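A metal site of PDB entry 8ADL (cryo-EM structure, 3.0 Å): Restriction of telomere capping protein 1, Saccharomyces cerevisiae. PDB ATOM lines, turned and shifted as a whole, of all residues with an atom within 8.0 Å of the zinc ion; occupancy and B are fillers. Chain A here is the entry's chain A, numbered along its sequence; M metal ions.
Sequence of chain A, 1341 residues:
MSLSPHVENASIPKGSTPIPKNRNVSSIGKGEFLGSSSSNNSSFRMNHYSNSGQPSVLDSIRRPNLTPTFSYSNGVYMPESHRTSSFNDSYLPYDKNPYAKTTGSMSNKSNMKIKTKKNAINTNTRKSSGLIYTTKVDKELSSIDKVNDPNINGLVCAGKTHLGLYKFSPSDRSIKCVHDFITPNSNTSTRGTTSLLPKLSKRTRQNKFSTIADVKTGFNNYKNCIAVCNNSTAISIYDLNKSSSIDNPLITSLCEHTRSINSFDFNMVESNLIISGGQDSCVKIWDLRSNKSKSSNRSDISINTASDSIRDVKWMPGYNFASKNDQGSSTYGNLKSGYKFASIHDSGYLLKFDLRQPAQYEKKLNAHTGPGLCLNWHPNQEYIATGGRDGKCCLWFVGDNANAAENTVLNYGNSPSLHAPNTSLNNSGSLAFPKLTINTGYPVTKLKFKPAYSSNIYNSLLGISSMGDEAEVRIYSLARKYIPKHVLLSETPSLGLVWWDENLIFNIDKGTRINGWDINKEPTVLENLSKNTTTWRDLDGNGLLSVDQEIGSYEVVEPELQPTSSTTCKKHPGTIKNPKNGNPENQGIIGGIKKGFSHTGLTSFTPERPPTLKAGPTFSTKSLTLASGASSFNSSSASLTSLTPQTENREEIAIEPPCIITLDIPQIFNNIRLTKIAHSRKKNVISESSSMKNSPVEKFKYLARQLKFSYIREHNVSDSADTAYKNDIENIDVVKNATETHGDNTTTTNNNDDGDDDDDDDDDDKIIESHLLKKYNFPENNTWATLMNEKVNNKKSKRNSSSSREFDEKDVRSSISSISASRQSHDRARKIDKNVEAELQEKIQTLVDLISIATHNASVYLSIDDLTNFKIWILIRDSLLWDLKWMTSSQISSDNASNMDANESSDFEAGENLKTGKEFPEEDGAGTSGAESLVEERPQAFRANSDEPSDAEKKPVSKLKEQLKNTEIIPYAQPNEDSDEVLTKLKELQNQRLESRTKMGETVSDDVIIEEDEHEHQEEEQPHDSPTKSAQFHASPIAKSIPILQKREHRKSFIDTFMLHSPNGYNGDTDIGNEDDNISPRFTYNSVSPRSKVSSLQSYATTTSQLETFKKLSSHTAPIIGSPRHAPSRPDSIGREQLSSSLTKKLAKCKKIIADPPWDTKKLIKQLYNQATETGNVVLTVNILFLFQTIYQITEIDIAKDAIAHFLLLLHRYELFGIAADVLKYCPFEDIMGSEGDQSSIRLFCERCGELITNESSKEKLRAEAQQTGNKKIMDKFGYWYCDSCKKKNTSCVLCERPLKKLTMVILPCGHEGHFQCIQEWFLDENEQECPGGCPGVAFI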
ATOM      1  N   PHE A1245      -2.325  -0.745  31.732  1.00  0.00           N
ATOM      2  CA  PHE A1245      -1.889   0.333  30.855  1.00  0.00           C
ATOM      3  C   PHE A1245      -2.508   0.135  29.482  1.00  0.00           C
ATOM      4  O   PHE A1245      -2.797  -0.998  29.070  1.00  0.00           O
ATOM      5  CB  PHE A1245      -0.371   0.380  30.749  1.00  0.00           C
ATOM      6  CG  PHE A1245       0.321   0.780  32.020  1.00  0.00           C
ATOM      7  CD1 PHE A1245       0.466   2.123  32.340  1.00  0.00           C
ATOM      8  CD2 PHE A1245       0.830  -0.175  32.885  1.00  0.00           C
ATOM      9  CE1 PHE A1245       1.109   2.496  33.508  1.00  0.00           C
ATOM     10  CE2 PHE A1245       1.462   0.194  34.044  1.00  0.00           C
ATOM     11  CZ  PHE A1245       1.607   1.537  34.364  1.00  0.00           C
ATOM     12  N   CYS A1246      -2.729   1.238  28.778  1.00  0.00           N
ATOM     13  CA  CYS A1246      -3.381   1.177  27.476  1.00  0.00           C
ATOM     14  C   CYS A1246      -2.460   0.533  26.445  1.00  0.00           C
ATOM     15  O   CYS A1246      -1.249   0.757  26.442  1.00  0.00           O
ATOM     16  CB  CYS A1246      -3.791   2.568  27.007  1.00  0.00           C
ATOM     17  SG  CYS A1246      -5.087   2.536  25.744  1.00  0.00           S
ATOM     18  N   GLU A1247      -3.054  -0.275  25.570  1.00  0.00           N
ATOM     19  CA  GLU A1247      -2.304  -0.926  24.496  1.00  0.00           C
ATOM     20  C   GLU A1247      -1.934   0.016  23.363  1.00  0.00           C
ATOM     21  O   GLU A1247      -1.112  -0.367  22.512  1.00  0.00           O
ATOM     22  CB  GLU A1247      -3.124  -2.089  23.937  1.00  0.00           C
ATOM     23  CG  GLU A1247      -4.541  -1.715  23.534  1.00  0.00           C
ATOM     24  CD  GLU A1247      -5.206  -2.775  22.698  1.00  0.00           C
ATOM     25  OE1 GLU A1247      -4.517  -3.742  22.294  1.00  0.00           O
ATOM     26  OE2 GLU A1247      -6.419  -2.663  22.431  1.00  0.00           O
ATOM     27  N   ARG A1248      -2.500   1.221  23.328  1.00  0.00           N
ATOM     28  CA  ARG A1248      -2.250   2.171  22.246  1.00  0.00           C
ATOM     29  C   ARG A1248      -1.412   3.363  22.686  1.00  0.00           C
ATOM     30  O   ARG A1248      -0.452   3.726  21.991  1.00  0.00           O
ATOM     31  CB  ARG A1248      -3.582   2.656  21.674  1.00  0.00           C
ATOM     32  CG  ARG A1248      -4.294   1.641  20.794  1.00  0.00           C
ATOM     33  CD  ARG A1248      -5.528   2.247  20.161  1.00  0.00           C
ATOM     34  NE  ARG A1248      -5.325   3.642  19.794  1.00  0.00           N
ATOM     35  CZ  ARG A1248      -6.302   4.525  19.618  1.00  0.00           C
ATOM     36  NH1 ARG A1248      -7.571   4.194  19.778  1.00  0.00           N
ATOM     37  NH2 ARG A1248      -5.988   5.775  19.285  1.00  0.00           N
ATOM     38  N   CYS A1249      -1.743   3.983  23.817  1.00  0.00           N
ATOM     39  CA  CYS A1249      -1.051   5.181  24.260  1.00  0.00           C
ATOM     40  C   CYS A1249      -0.080   4.935  25.398  1.00  0.00           C
ATOM     41  O   CYS A1249       0.882   5.703  25.562  1.00  0.00           O
ATOM     42  CB  CYS A1249      -2.070   6.245  24.690  1.00  0.00           C
ATOM     43  SG  CYS A1249      -3.121   5.749  26.069  1.00  0.00           S
ATOM     44  N   GLY A1250      -0.284   3.883  26.197  1.00  0.00           N
ATOM     45  CA  GLY A1250       0.636   3.540  27.255  1.00  0.00           C
ATOM     46  C   GLY A1250       0.338   4.148  28.608  1.00  0.00           C
ATOM     47  O   GLY A1250       0.978   3.766  29.598  1.00  0.00           O
ATOM     48  N   GLU A1251      -0.613   5.076  28.697  1.00  0.00           N
ATOM     49  CA  GLU A1251      -0.985   5.616  29.998  1.00  0.00           C
ATOM     50  C   GLU A1251      -1.874   4.634  30.750  1.00  0.00           C
ATOM     51  O   GLU A1251      -2.476   3.721  30.168  1.00  0.00           O
ATOM     52  CB  GLU A1251      -1.695   6.967  29.850  1.00  0.00           C
ATOM     53  CG  GLU A1251      -0.758   8.153  29.711  1.00  0.00           C
ATOM     54  CD  GLU A1251      -0.360   8.444  28.278  1.00  0.00           C
ATOM     55  OE1 GLU A1251      -0.912   7.789  27.373  1.00  0.00           O
ATOM     56  OE2 GLU A1251       0.504   9.321  28.066  1.00  0.00           O
ATOM     57  N   LEU A1252      -1.944   4.815  32.061  1.00  0.00           N
ATOM     58  CA  LEU A1252      -2.703   3.911  32.909  1.00  0.00           C
ATOM     59  C   LEU A1252      -4.202   4.086  32.711  1.00  0.00           C
ATOM     60  O   LEU A1252      -4.703   5.207  32.632  1.00  0.00           O
ATOM     61  CB  LEU A1252      -2.335   4.133  34.384  1.00  0.00           C
ATOM     62  CG  LEU A1252      -2.867   3.100  35.385  1.00  0.00           C
ATOM     63  CD1 LEU A1252      -2.009   1.857  35.368  1.00  0.00           C
ATOM     64  CD2 LEU A1252      -2.928   3.691  36.779  1.00  0.00           C
ATOM     65  N   ILE A1253      -4.914   2.967  32.633  1.00  0.00           N
ATOM     66  CA  ILE A1253      -6.366   2.986  32.507  1.00  0.00           C
ATOM     67  C   ILE A1253      -6.981   3.195  33.888  1.00  0.00           C
ATOM     68  O   ILE A1253      -7.214   2.231  34.623  1.00  0.00           O
ATOM     69  CB  ILE A1253      -6.902   1.703  31.849  1.00  0.00           C
ATOM     70  CG1 ILE A1253      -6.191   1.434  30.531  1.00  0.00           C
ATOM     71  CG2 ILE A1253      -8.406   1.799  31.624  1.00  0.00           C
ATOM     72  CD1 ILE A1253      -6.523   2.446  29.466  1.00  0.00           C
ATOM     73  N   ASN A1255      -9.559   6.008  34.094  1.00  0.00           N
ATOM     74  CA  ASN A1255     -10.869   6.449  33.608  1.00  0.00           C
ATOM     75  C   ASN A1255     -11.625   7.282  34.652  1.00  0.00           C
ATOM     76  O   ASN A1255     -12.804   7.073  34.915  1.00  0.00           O
ATOM     77  CB  ASN A1255     -11.709   5.255  33.158  1.00  0.00           C
ATOM     78  CG  ASN A1255     -11.170   4.606  31.900  1.00  0.00           C
ATOM     79  OD1 ASN A1255     -10.278   5.145  31.243  1.00  0.00           O
ATOM     80  ND2 ASN A1255     -11.715   3.449  31.548  1.00  0.00           N
ATOM     81  N   TYR A1282     -12.003   0.700  27.934  1.00  0.00           N
ATOM     82  CA  TYR A1282     -11.791   1.861  27.086  1.00  0.00           C
ATOM     83  C   TYR A1282     -10.811   2.812  27.766  1.00  0.00           C
ATOM     84  O   TYR A1282     -10.653   2.808  28.984  1.00  0.00           O
ATOM     85  CB  TYR A1282     -13.110   2.574  26.769  1.00  0.00           C
ATOM     86  CG  TYR A1282     -13.879   3.074  27.982  1.00  0.00           C
ATOM     87  CD1 TYR A1282     -14.779   2.251  28.627  1.00  0.00           C
ATOM     88  CD2 TYR A1282     -13.701   4.365  28.460  1.00  0.00           C
ATOM     89  CE1 TYR A1282     -15.488   2.699  29.732  1.00  0.00           C
ATOM     90  CE2 TYR A1282     -14.400   4.815  29.564  1.00  0.00           C
ATOM     91  CZ  TYR A1282     -15.300   3.979  30.190  1.00  0.00           C
ATOM     92  OH  TYR A1282     -15.998   4.417  31.285  1.00  0.00           O
ATOM     93  N   CYS A1283     -10.161   3.631  26.953  1.00  0.00           N
ATOM     94  CA  CYS A1283      -9.223   4.635  27.426  1.00  0.00           C
ATOM     95  C   CYS A1283      -9.822   6.017  27.231  1.00  0.00           C
ATOM     96  O   CYS A1283     -10.390   6.314  26.167  1.00  0.00           O
ATOM     97  CB  CYS A1283      -7.879   4.539  26.709  1.00  0.00           C
ATOM     98  SG  CYS A1283      -6.616   5.616  27.402  1.00  0.00           S
ATOM     99  N   ASP A1284      -9.715   6.868  28.249  1.00  0.00           N
ATOM    100  CA  ASP A1284     -10.149   8.249  28.119  1.00  0.00           C
ATOM    101  C   ASP A1284      -9.084   9.155  27.536  1.00  0.00           C
ATOM    102  O   ASP A1284      -9.418  10.195  26.955  1.00  0.00           O
ATOM    103  CB  ASP A1284     -10.584   8.784  29.488  1.00  0.00           C
ATOM    104  CG  ASP A1284     -12.046   8.517  29.778  1.00  0.00           C
ATOM    105  OD1 ASP A1284     -12.801   8.220  28.833  1.00  0.00           O
ATOM    106  OD2 ASP A1284     -12.438   8.588  30.966  1.00  0.00           O
ATOM    107  N   SER A1285      -7.809   8.790  27.676  1.00  0.00           N
ATOM    108  CA  SER A1285      -6.730   9.651  27.191  1.00  0.00           C
ATOM    109  C   SER A1285      -6.639   9.611  25.671  1.00  0.00           C
ATOM    110  O   SER A1285      -6.530  10.659  25.015  1.00  0.00           O
ATOM    111  CB  SER A1285      -5.404   9.223  27.816  1.00  0.00           C
ATOM    112  OG  SER A1285      -5.443   9.332  29.228  1.00  0.00           O
ATOM    113  N   CYS A1286      -6.690   8.420  25.082  1.00  0.00           N
ATOM    114  CA  CYS A1286      -6.536   8.241  23.640  1.00  0.00           C
ATOM    115  C   CYS A1286      -7.839   7.902  22.928  1.00  0.00           C
ATOM    116  O   CYS A1286      -7.809   7.643  21.726  1.00  0.00           O
ATOM    117  CB  CYS A1286      -5.494   7.163  23.353  1.00  0.00           C
ATOM    118  SG  CYS A1286      -6.078   5.480  23.623  1.00  0.00           S
ATOM    119  N   LYS A1287      -8.969   7.886  23.653  1.00  0.00           N
ATOM    120  CA  LYS A1287     -10.305   7.603  23.098  1.00  0.00           C
ATOM    121  C   LYS A1287     -10.384   6.242  22.398  1.00  0.00           C
ATOM    122  O   LYS A1287     -10.986   6.114  21.338  1.00  0.00           O
ATOM    123  CB  LYS A1287     -10.766   8.717  22.171  1.00  0.00           C
ATOM    124  CG  LYS A1287     -10.821  10.088  22.822  1.00  0.00           C
ATOM    125  CD  LYS A1287     -11.767  10.092  24.014  1.00  0.00           C
ATOM    126  CE  LYS A1287     -12.005  11.502  24.533  1.00  0.00           C
ATOM    127  NZ  LYS A1287     -10.766  12.090  25.128  1.00  0.00           N
ATOM    128  N   LYS A1288      -9.763   5.226  22.998  1.00  0.00           N
ATOM    129  CA  LYS A1288      -9.946   3.858  22.503  1.00  0.00           C
ATOM    130  C   LYS A1288     -11.381   3.417  22.769  1.00  0.00           C
ATOM    131  O   LYS A1288     -11.909   3.618  23.867  1.00  0.00           O
ATOM    132  CB  LYS A1288      -8.967   2.900  23.169  1.00  0.00           C
ATOM    133  CG  LYS A1288      -9.085   1.462  22.649  1.00  0.00           C
ATOM    134  CD  LYS A1288      -8.040   0.532  23.243  1.00  0.00           C
ATOM    135  CE  LYS A1288      -8.364   0.198  24.686  1.00  0.00           C
ATOM    136  NZ  LYS A1288      -7.418  -0.815  25.243  1.00  0.00           N
HETATM  137 ZN    ZN M   1      -5.232   4.858  25.703  1.00  0.00          ZN
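The zinc ion is bound by the side-chain sulfur of Cys 1283 (2.3 Å), the side-chain sulfur of Cys 1249 (2.3 Å), the side-chain sulfur of Cys 1246 (2.3 Å) and the side-chain sulfur of Cys 1286 (2.3 Å).
The backbone NH of Ser 1285 sits close to the side-chain sulfur of Cys 1283. The side-chain sulfur (SG) of Cys 1246 lies close to the backbone NH (N) of Arg 1248 (3.8 Å). The side-chain sulfur of Cys 1286 sits close to the backbone NH of Lys 1288 (3.7 Å). The backbone NH of Cys 1246 is in hydrogen-bond range of the backbone carbonyl oxygen of Glu 1251, 2.9 Å away. The side-chain sulfur (SG) of Cys 1249 lies close to the side-chain carboxylate (OE1) of Glu 1251. N of Lys 1288 is in hydrogen-bond range of O of Cys 1283 (3.4 Å).
Four residues have an atom within 4 Å of the zinc ion: Cys 1246, Cys 1249, Cys 1283 and Cys 1286. The nearest printed residue that does not touch the zinc ion is Ile 1253 (4.7 Å).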
